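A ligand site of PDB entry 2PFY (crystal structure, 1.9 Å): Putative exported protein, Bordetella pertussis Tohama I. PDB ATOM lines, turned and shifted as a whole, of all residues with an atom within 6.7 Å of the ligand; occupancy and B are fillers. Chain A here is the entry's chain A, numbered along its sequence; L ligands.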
ATOM      1  N   GLU A   9     -10.814  11.286   8.214  1.00  0.00           N
ATOM      2  CA  GLU A   9     -11.499  10.031   7.890  1.00  0.00           C
ATOM      3  C   GLU A   9     -10.897   8.762   8.559  1.00  0.00           C
ATOM      4  O   GLU A   9     -11.592   7.872   9.054  1.00  0.00           O
ATOM      5  CB  GLU A   9     -11.383   9.889   6.387  1.00  0.00           C
ATOM      6  CG  GLU A   9     -12.578   9.445   5.713  1.00  0.00           C
ATOM      7  CD  GLU A   9     -12.331   9.275   4.247  1.00  0.00           C
ATOM      8  OE1 GLU A   9     -13.112   9.799   3.451  1.00  0.00           O
ATOM      9  OE2 GLU A   9     -11.359   8.592   3.890  1.00  0.00           O
ATOM     10  N   GLN A  10      -9.573   8.693   8.558  1.00  0.00           N
ATOM     11  CA  GLN A  10      -8.847   7.475   8.866  1.00  0.00           C
ATOM     12  C   GLN A  10      -8.239   7.509  10.266  1.00  0.00           C
ATOM     13  O   GLN A  10      -8.070   8.607  10.851  1.00  0.00           O
ATOM     14  CB  GLN A  10      -7.778   7.293   7.789  1.00  0.00           C
ATOM     15  CG  GLN A  10      -8.353   7.262   6.334  1.00  0.00           C
ATOM     16  CD  GLN A  10      -9.319   6.102   6.149  1.00  0.00           C
ATOM     17  OE1 GLN A  10      -9.132   5.025   6.742  1.00  0.00           O
ATOM     18  NE2 GLN A  10     -10.374   6.311   5.354  1.00  0.00           N
ATOM     19  N   ASN A  14      -2.904   6.011  10.003  1.00  0.00           N
ATOM     20  CA  ASN A  14      -2.922   6.304   8.590  1.00  0.00           C
ATOM     21  C   ASN A  14      -2.099   7.524   8.251  1.00  0.00           C
ATOM     22  O   ASN A  14      -2.144   8.499   8.981  1.00  0.00           O
ATOM     23  CB  ASN A  14      -4.388   6.493   8.135  1.00  0.00           C
ATOM     24  CG  ASN A  14      -4.487   6.947   6.712  1.00  0.00           C
ATOM     25  OD1 ASN A  14      -4.479   8.171   6.422  1.00  0.00           O
ATOM     26  ND2 ASN A  14      -4.607   5.979   5.789  1.00  0.00           N
ATOM     27  N   ARG A  48     -17.463   9.418   6.142  1.00  0.00           N
ATOM     28  CA  ARG A  48     -17.117   9.868   4.804  1.00  0.00           C
ATOM     29  C   ARG A  48     -18.262  10.552   4.028  1.00  0.00           C
ATOM     30  O   ARG A  48     -18.046  11.612   3.495  1.00  0.00           O
ATOM     31  CB  ARG A  48     -16.535   8.708   3.979  1.00  0.00           C
ATOM     32  CG  ARG A  48     -16.249   9.024   2.531  1.00  0.00           C
ATOM     33  CD  ARG A  48     -15.592   7.806   1.816  1.00  0.00           C
ATOM     34  NE  ARG A  48     -14.198   7.617   2.208  1.00  0.00           N
ATOM     35  CZ  ARG A  48     -13.547   6.456   2.103  1.00  0.00           C
ATOM     36  NH1 ARG A  48     -14.175   5.395   1.601  1.00  0.00           N
ATOM     37  NH2 ARG A  48     -12.265   6.358   2.474  1.00  0.00           N
ATOM     38  N   LEU A  66     -12.207  11.579   1.261  1.00  0.00           N
ATOM     39  CA  LEU A  66     -11.955  11.030  -0.049  1.00  0.00           C
ATOM     40  C   LEU A  66     -12.654  11.927  -1.065  1.00  0.00           C
ATOM     41  O   LEU A  66     -13.867  12.167  -0.956  1.00  0.00           O
ATOM     42  CB  LEU A  66     -12.566   9.608  -0.101  1.00  0.00           C
ATOM     43  CG  LEU A  66     -12.321   8.800  -1.380  1.00  0.00           C
ATOM     44  CD1 LEU A  66     -10.837   8.343  -1.442  1.00  0.00           C
ATOM     45  CD2 LEU A  66     -13.281   7.602  -1.473  1.00  0.00           C
ATOM     46  N   TRP A 120      -3.944   8.671  -1.822  1.00  0.00           N
ATOM     47  CA  TRP A 120      -3.772   7.304  -1.332  1.00  0.00           C
ATOM     48  C   TRP A 120      -2.752   6.602  -2.269  1.00  0.00           C
ATOM     49  O   TRP A 120      -2.451   7.096  -3.350  1.00  0.00           O
ATOM     50  CB  TRP A 120      -5.119   6.561  -1.443  1.00  0.00           C
ATOM     51  CG  TRP A 120      -6.078   6.970  -0.390  1.00  0.00           C
ATOM     52  CD1 TRP A 120      -7.057   7.945  -0.465  1.00  0.00           C
ATOM     53  CD2 TRP A 120      -6.180   6.395   0.908  1.00  0.00           C
ATOM     54  NE1 TRP A 120      -7.765   7.982   0.711  1.00  0.00           N
ATOM     55  CE2 TRP A 120      -7.251   7.041   1.575  1.00  0.00           C
ATOM     56  CE3 TRP A 120      -5.454   5.375   1.579  1.00  0.00           C
ATOM     57  CZ2 TRP A 120      -7.626   6.704   2.880  1.00  0.00           C
ATOM     58  CZ3 TRP A 120      -5.836   5.050   2.888  1.00  0.00           C
ATOM     59  CH2 TRP A 120      -6.909   5.701   3.515  1.00  0.00           C
ATOM     60  N   PRO A 121      -2.204   5.447  -1.816  1.00  0.00           N
ATOM     61  CA  PRO A 121      -1.441   4.620  -2.740  1.00  0.00           C
ATOM     62  C   PRO A 121      -2.370   3.943  -3.757  1.00  0.00           C
ATOM     63  O   PRO A 121      -3.602   4.016  -3.630  1.00  0.00           O
ATOM     64  CB  PRO A 121      -0.725   3.603  -1.811  1.00  0.00           C
ATOM     65  CG  PRO A 121      -0.878   4.178  -0.377  1.00  0.00           C
ATOM     66  CD  PRO A 121      -2.226   4.883  -0.454  1.00  0.00           C
ATOM     67  N   PRO A 122      -1.793   3.321  -4.803  1.00  0.00           N
ATOM     68  CA  PRO A 122      -2.585   2.634  -5.822  1.00  0.00           C
ATOM     69  C   PRO A 122      -3.450   1.516  -5.242  1.00  0.00           C
ATOM     70  O   PRO A 122      -3.084   0.903  -4.225  1.00  0.00           O
ATOM     71  CB  PRO A 122      -1.522   2.055  -6.757  1.00  0.00           C
ATOM     72  CG  PRO A 122      -0.332   2.974  -6.575  1.00  0.00           C
ATOM     73  CD  PRO A 122      -0.344   3.279  -5.091  1.00  0.00           C
ATOM     74  N   GLN A 123      -4.601   1.240  -5.878  1.00  0.00           N
ATOM     75  CA  GLN A 123      -5.574   0.307  -5.297  1.00  0.00           C
ATOM     76  C   GLN A 123      -5.310  -1.115  -5.788  1.00  0.00           C
ATOM     77  O   GLN A 123      -5.303  -1.354  -6.994  1.00  0.00           O
ATOM     78  CB  GLN A 123      -7.007   0.718  -5.664  1.00  0.00           C
ATOM     79  CG  GLN A 123      -7.354   2.192  -5.324  1.00  0.00           C
ATOM     80  CD  GLN A 123      -7.417   2.417  -3.812  1.00  0.00           C
ATOM     81  OE1 GLN A 123      -6.490   2.953  -3.204  1.00  0.00           O
ATOM     82  NE2 GLN A 123      -8.482   1.976  -3.220  1.00  0.00           N
ATOM     83  N   ARG A 143     -16.518  -5.448  -1.303  1.00  0.00           N
ATOM     84  CA  ARG A 143     -16.592  -4.106  -0.703  1.00  0.00           C
ATOM     85  C   ARG A 143     -16.503  -2.991  -1.722  1.00  0.00           C
ATOM     86  O   ARG A 143     -15.591  -2.973  -2.559  1.00  0.00           O
ATOM     87  CB  ARG A 143     -15.465  -3.915   0.325  1.00  0.00           C
ATOM     88  CG  ARG A 143     -15.484  -2.495   0.974  1.00  0.00           C
ATOM     89  CD  ARG A 143     -14.285  -2.237   1.802  1.00  0.00           C
ATOM     90  NE  ARG A 143     -14.359  -0.850   2.298  1.00  0.00           N
ATOM     91  CZ  ARG A 143     -13.366   0.023   2.244  1.00  0.00           C
ATOM     92  NH1 ARG A 143     -12.177  -0.357   1.785  1.00  0.00           N
ATOM     93  NH2 ARG A 143     -13.544   1.287   2.696  1.00  0.00           N
ATOM     94  N   TYR A 145     -16.619   1.491  -1.710  1.00  0.00           N
ATOM     95  CA  TYR A 145     -16.451   2.574  -0.727  1.00  0.00           C
ATOM     96  C   TYR A 145     -16.811   3.954  -1.251  1.00  0.00           C
ATOM     97  O   TYR A 145     -16.576   4.978  -0.594  1.00  0.00           O
ATOM     98  CB  TYR A 145     -15.042   2.554  -0.103  1.00  0.00           C
ATOM     99  CG  TYR A 145     -13.889   2.718  -1.060  1.00  0.00           C
ATOM    100  CD1 TYR A 145     -13.696   3.911  -1.767  1.00  0.00           C
ATOM    101  CD2 TYR A 145     -12.941   1.687  -1.229  1.00  0.00           C
ATOM    102  CE1 TYR A 145     -12.651   4.064  -2.619  1.00  0.00           C
ATOM    103  CE2 TYR A 145     -11.879   1.832  -2.104  1.00  0.00           C
ATOM    104  CZ  TYR A 145     -11.736   3.023  -2.807  1.00  0.00           C
ATOM    105  OH  TYR A 145     -10.696   3.231  -3.681  1.00  0.00           O
ATOM    106  N   VAL A 163     -19.047  -0.343   2.369  1.00  0.00           N
ATOM    107  CA  VAL A 163     -18.578  -0.431   3.764  1.00  0.00           C
ATOM    108  C   VAL A 163     -17.527   0.658   3.943  1.00  0.00           C
ATOM    109  O   VAL A 163     -16.573   0.727   3.170  1.00  0.00           O
ATOM    110  CB  VAL A 163     -17.960  -1.828   4.106  1.00  0.00           C
ATOM    111  CG1 VAL A 163     -17.488  -1.865   5.549  1.00  0.00           C
ATOM    112  CG2 VAL A 163     -18.978  -2.967   3.877  1.00  0.00           C
ATOM    113  N   GLN A 164     -17.730   1.511   4.946  1.00  0.00           N
ATOM    114  CA  GLN A 164     -16.791   2.610   5.146  1.00  0.00           C
ATOM    115  C   GLN A 164     -15.569   2.030   5.839  1.00  0.00           C
ATOM    116  O   GLN A 164     -15.667   0.960   6.483  1.00  0.00           O
ATOM    117  CB  GLN A 164     -17.437   3.744   5.972  1.00  0.00           C
ATOM    118  CG  GLN A 164     -18.658   4.466   5.282  1.00  0.00           C
ATOM    119  CD  GLN A 164     -18.345   4.968   3.890  1.00  0.00           C
ATOM    120  OE1 GLN A 164     -17.204   5.355   3.584  1.00  0.00           O
ATOM    121  NE2 GLN A 164     -19.362   4.961   3.005  1.00  0.00           N
ATOM    122  N   THR A 165     -14.440   2.728   5.775  1.00  0.00           N
ATOM    123  CA  THR A 165     -13.151   2.135   6.178  1.00  0.00           C
ATOM    124  C   THR A 165     -13.080   1.540   7.603  1.00  0.00           C
ATOM    125  O   THR A 165     -12.555   0.427   7.786  1.00  0.00           O
ATOM    126  CB  THR A 165     -11.951   3.081   5.878  1.00  0.00           C
ATOM    127  OG1 THR A 165     -12.295   4.027   4.827  1.00  0.00           O
ATOM    128  CG2 THR A 165     -10.708   2.237   5.435  1.00  0.00           C
ATOM    129  N   VAL A 168     -14.569  -2.084   8.067  1.00  0.00           N
ATOM    130  CA  VAL A 168     -14.080  -3.170   7.177  1.00  0.00           C
ATOM    131  C   VAL A 168     -13.815  -4.466   7.961  1.00  0.00           C
ATOM    132  O   VAL A 168     -14.334  -5.508   7.568  1.00  0.00           O
ATOM    133  CB  VAL A 168     -12.900  -2.740   6.315  1.00  0.00           C
ATOM    134  CG1 VAL A 168     -12.124  -3.967   5.687  1.00  0.00           C
ATOM    135  CG2 VAL A 168     -13.334  -1.762   5.254  1.00  0.00           C
ATOM    136  N   MET A 180     -12.117  -7.158  -1.298  1.00  0.00           N
ATOM    137  CA  MET A 180     -12.182  -5.690  -1.392  1.00  0.00           C
ATOM    138  C   MET A 180     -11.114  -5.150  -2.307  1.00  0.00           C
ATOM    139  O   MET A 180     -10.208  -5.890  -2.767  1.00  0.00           O
ATOM    140  CB  MET A 180     -12.092  -5.081   0.022  1.00  0.00           C
ATOM    141  CG  MET A 180     -10.810  -5.391   0.731  1.00  0.00           C
ATOM    142  SD  MET A 180     -10.646  -4.265   2.290  1.00  0.00           S
ATOM    143  CE  MET A 180      -8.815  -4.932   2.958  1.00  0.00           C
ATOM    144  N   LEU A 181     -11.221  -3.858  -2.561  1.00  0.00           N
ATOM    145  CA  LEU A 181     -10.254  -3.156  -3.373  1.00  0.00           C
ATOM    146  C   LEU A 181      -9.880  -1.924  -2.575  1.00  0.00           C
ATOM    147  O   LEU A 181     -10.772  -1.145  -2.181  1.00  0.00           O
ATOM    148  CB  LEU A 181     -10.858  -2.737  -4.719  1.00  0.00           C
ATOM    149  CG  LEU A 181      -9.956  -1.816  -5.561  1.00  0.00           C
ATOM    150  CD1 LEU A 181      -9.805  -2.268  -7.038  1.00  0.00           C
ATOM    151  CD2 LEU A 181     -10.483  -0.366  -5.516  1.00  0.00           C
ATOM    152  N   THR A 182      -8.586  -1.784  -2.312  1.00  0.00           N
ATOM    153  CA  THR A 182      -8.076  -0.672  -1.493  1.00  0.00           C
ATOM    154  C   THR A 182      -6.564  -0.685  -1.558  1.00  0.00           C
ATOM    155  O   THR A 182      -5.977  -1.664  -2.060  1.00  0.00           O
ATOM    156  CB  THR A 182      -8.623  -0.684  -0.012  1.00  0.00           C
ATOM    157  OG1 THR A 182      -8.327   0.564   0.625  1.00  0.00           O
ATOM    158  CG2 THR A 182      -8.050  -1.865   0.860  1.00  0.00           C
ATOM    159  N   SER A 183      -5.933   0.371  -1.016  1.00  0.00           N
ATOM    160  CA  SER A 183      -4.492   0.507  -1.041  1.00  0.00           C
ATOM    161  C   SER A 183      -3.851  -0.438  -0.024  1.00  0.00           C
ATOM    162  O   SER A 183      -4.519  -0.939   0.929  1.00  0.00           O
ATOM    163  CB  SER A 183      -4.084   1.933  -0.689  1.00  0.00           C
ATOM    164  OG  SER A 183      -4.543   2.210   0.631  1.00  0.00           O
ATOM    165  N   PRO A 184      -2.530  -0.631  -0.175  1.00  0.00           N
ATOM    166  CA  PRO A 184      -1.782  -1.273   0.904  1.00  0.00           C
ATOM    167  C   PRO A 184      -1.750  -0.438   2.191  1.00  0.00           C
ATOM    168  O   PRO A 184      -1.515  -0.983   3.271  1.00  0.00           O
ATOM    169  CB  PRO A 184      -0.378  -1.464   0.305  1.00  0.00           C
ATOM    170  CG  PRO A 184      -0.254  -0.363  -0.786  1.00  0.00           C
ATOM    171  CD  PRO A 184      -1.685  -0.310  -1.349  1.00  0.00           C
ATOM    172  N   ALA A 185      -2.042   0.877   2.116  1.00  0.00           N
ATOM    173  CA  ALA A 185      -2.093   1.685   3.353  1.00  0.00           C
ATOM    174  C   ALA A 185      -3.249   1.252   4.259  1.00  0.00           C
ATOM    175  O   ALA A 185      -3.081   1.096   5.465  1.00  0.00           O
ATOM    176  CB  ALA A 185      -2.222   3.175   3.030  1.00  0.00           C
ATOM    177  N   THR A 186      -4.435   1.096   3.659  1.00  0.00           N
ATOM    178  CA  THR A 186      -5.614   0.595   4.395  1.00  0.00           C
ATOM    179  C   THR A 186      -5.362  -0.844   4.850  1.00  0.00           C
ATOM    180  O   THR A 186      -5.744  -1.248   5.958  1.00  0.00           O
ATOM    181  CB  THR A 186      -6.872   0.695   3.533  1.00  0.00           C
ATOM    182  OG1 THR A 186      -7.194   2.087   3.386  1.00  0.00           O
ATOM    183  CG2 THR A 186      -8.075  -0.034   4.189  1.00  0.00           C
ATOM    184  N   ASP A 189      -3.073  -0.195   7.902  1.00  0.00           N
ATOM    185  CA  ASP A 189      -3.951   0.488   8.894  1.00  0.00           C
ATOM    186  C   ASP A 189      -4.883  -0.525   9.593  1.00  0.00           C
ATOM    187  O   ASP A 189      -5.013  -0.522  10.830  1.00  0.00           O
ATOM    188  CB  ASP A 189      -4.878   1.535   8.225  1.00  0.00           C
ATOM    189  CG  ASP A 189      -4.129   2.702   7.548  1.00  0.00           C
ATOM    190  OD1 ASP A 189      -2.923   2.950   7.801  1.00  0.00           O
ATOM    191  OD2 ASP A 189      -4.809   3.406   6.749  1.00  0.00           O
ATOM    192  N   PHE A 205      -6.378   2.295  -9.699  1.00  0.00           N
ATOM    193  CA  PHE A 205      -6.379   3.736  -9.765  1.00  0.00           C
ATOM    194  C   PHE A 205      -5.738   4.309  -8.509  1.00  0.00           C
ATOM    195  O   PHE A 205      -5.333   3.580  -7.577  1.00  0.00           O
ATOM    196  CB  PHE A 205      -7.813   4.298  -9.968  1.00  0.00           C
ATOM    197  CG  PHE A 205      -8.797   3.853  -8.938  1.00  0.00           C
ATOM    198  CD1 PHE A 205      -9.015   4.631  -7.769  1.00  0.00           C
ATOM    199  CD2 PHE A 205      -9.462   2.642  -9.074  1.00  0.00           C
ATOM    200  CE1 PHE A 205      -9.917   4.216  -6.793  1.00  0.00           C
ATOM    201  CE2 PHE A 205     -10.379   2.207  -8.063  1.00  0.00           C
ATOM    202  CZ  PHE A 205     -10.607   2.996  -6.943  1.00  0.00           C
ATOM    203  N   PRO A 207      -6.822   7.090  -5.820  1.00  0.00           N
ATOM    204  CA  PRO A 207      -7.856   8.054  -5.449  1.00  0.00           C
ATOM    205  C   PRO A 207      -7.239   9.105  -4.534  1.00  0.00           C
ATOM    206  O   PRO A 207      -6.299   8.819  -3.769  1.00  0.00           O
ATOM    207  CB  PRO A 207      -8.921   7.200  -4.755  1.00  0.00           C
ATOM    208  CG  PRO A 207      -8.056   6.032  -4.077  1.00  0.00           C
ATOM    209  CD  PRO A 207      -6.869   5.853  -5.009  1.00  0.00           C
HETATM  210  N1  LIG L   1      -8.365   3.495   1.363  1.00  0.00           N
HETATM  211  C1  LIG L   1      -9.699   4.135   1.419  1.00  0.00           C
HETATM  212  C2  LIG L   1     -10.013   4.741   0.073  1.00  0.00           C
HETATM  213  C3  LIG L   1      -8.868   4.400  -0.822  1.00  0.00           C
HETATM  214  C4  LIG L   1      -7.891   3.662   0.044  1.00  0.00           C
HETATM  215  O1  LIG L   1      -6.779   3.296  -0.334  1.00  0.00           O
HETATM  216  C5  LIG L   1     -10.755   3.109   1.783  1.00  0.00           C
HETATM  217  O2  LIG L   1     -11.910   3.405   2.129  1.00  0.00           O
HETATM  218  O3  LIG L   1     -10.452   1.933   1.743  1.00  0.00           O
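N of Trp 120 sits at hydrogen-bond distance from O of Pro 207 (3.1 Å). The side-chain amide oxygen of Gln 123 lies close to the backbone carbonyl oxygen of Pro 121, at 3.1 Å. OH of Tyr 145 is in hydrogen-bond range of NE2 of Gln 123 (2.6 Å). The side-chain hydroxyl (OG1) of Thr 186 sits close to the side-chain hydroxyl (OG1) of Thr 182 (3.4 Å). The side-chain carboxylate (OE1) of Glu 9 lies within salt-bridge range of the guanidinium group (NE) of Arg 48. OE1 of Gln 123 sits at hydrogen-bond distance from N of Ser 183 (3.4 Å). NE2 of Gln 10 lies within hydrogen-bond range of OG1 of Thr 165 (3.0 Å). The side-chain hydroxyl (OG1) of Thr 165 is in hydrogen-bond range of the guanidinium group (NH2) of Arg 48.
CD1 of Leu 66 touches C2 of the ligand (3.99 Å). CE3 of Trp 120 touches O1 of the ligand (3.1 Å). OH of Tyr 145 touches C3 of the ligand (3.6 Å). Pro 207 touches the ligand. Of the 25 residues printed, 11 come within 4 Å of the ligand. The nearest printed residue that does not touch the ligand is Gln 10 (4.5 Å).
OE1 of Gln 123 lies close to O1 of the ligand. NH2 of Arg 143 lies within salt-bridge range of O2 of the ligand. An oxygen (O1) of the ligand lies close to the backbone NH (N) of Ser 183, 3.1 Å away. The side-chain hydroxyl of Ser 183 is in hydrogen-bond range of an oxygen (O1) of the ligand (2.7 Å). OG1 of Thr 186 sits at hydrogen-bond distance from N1 of the ligand (2.7 Å). The guanidinium group of Arg 48 lies within salt-bridge range of an oxygen (O2) of the ligand (3.0 Å). O3 of the ligand sits at hydrogen-bond distance from OG1 of Thr 182. The side-chain hydroxyl (OG1) of Thr 165 is in hydrogen-bond range of an oxygen (O2) of the ligand, at 2.8 Å.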
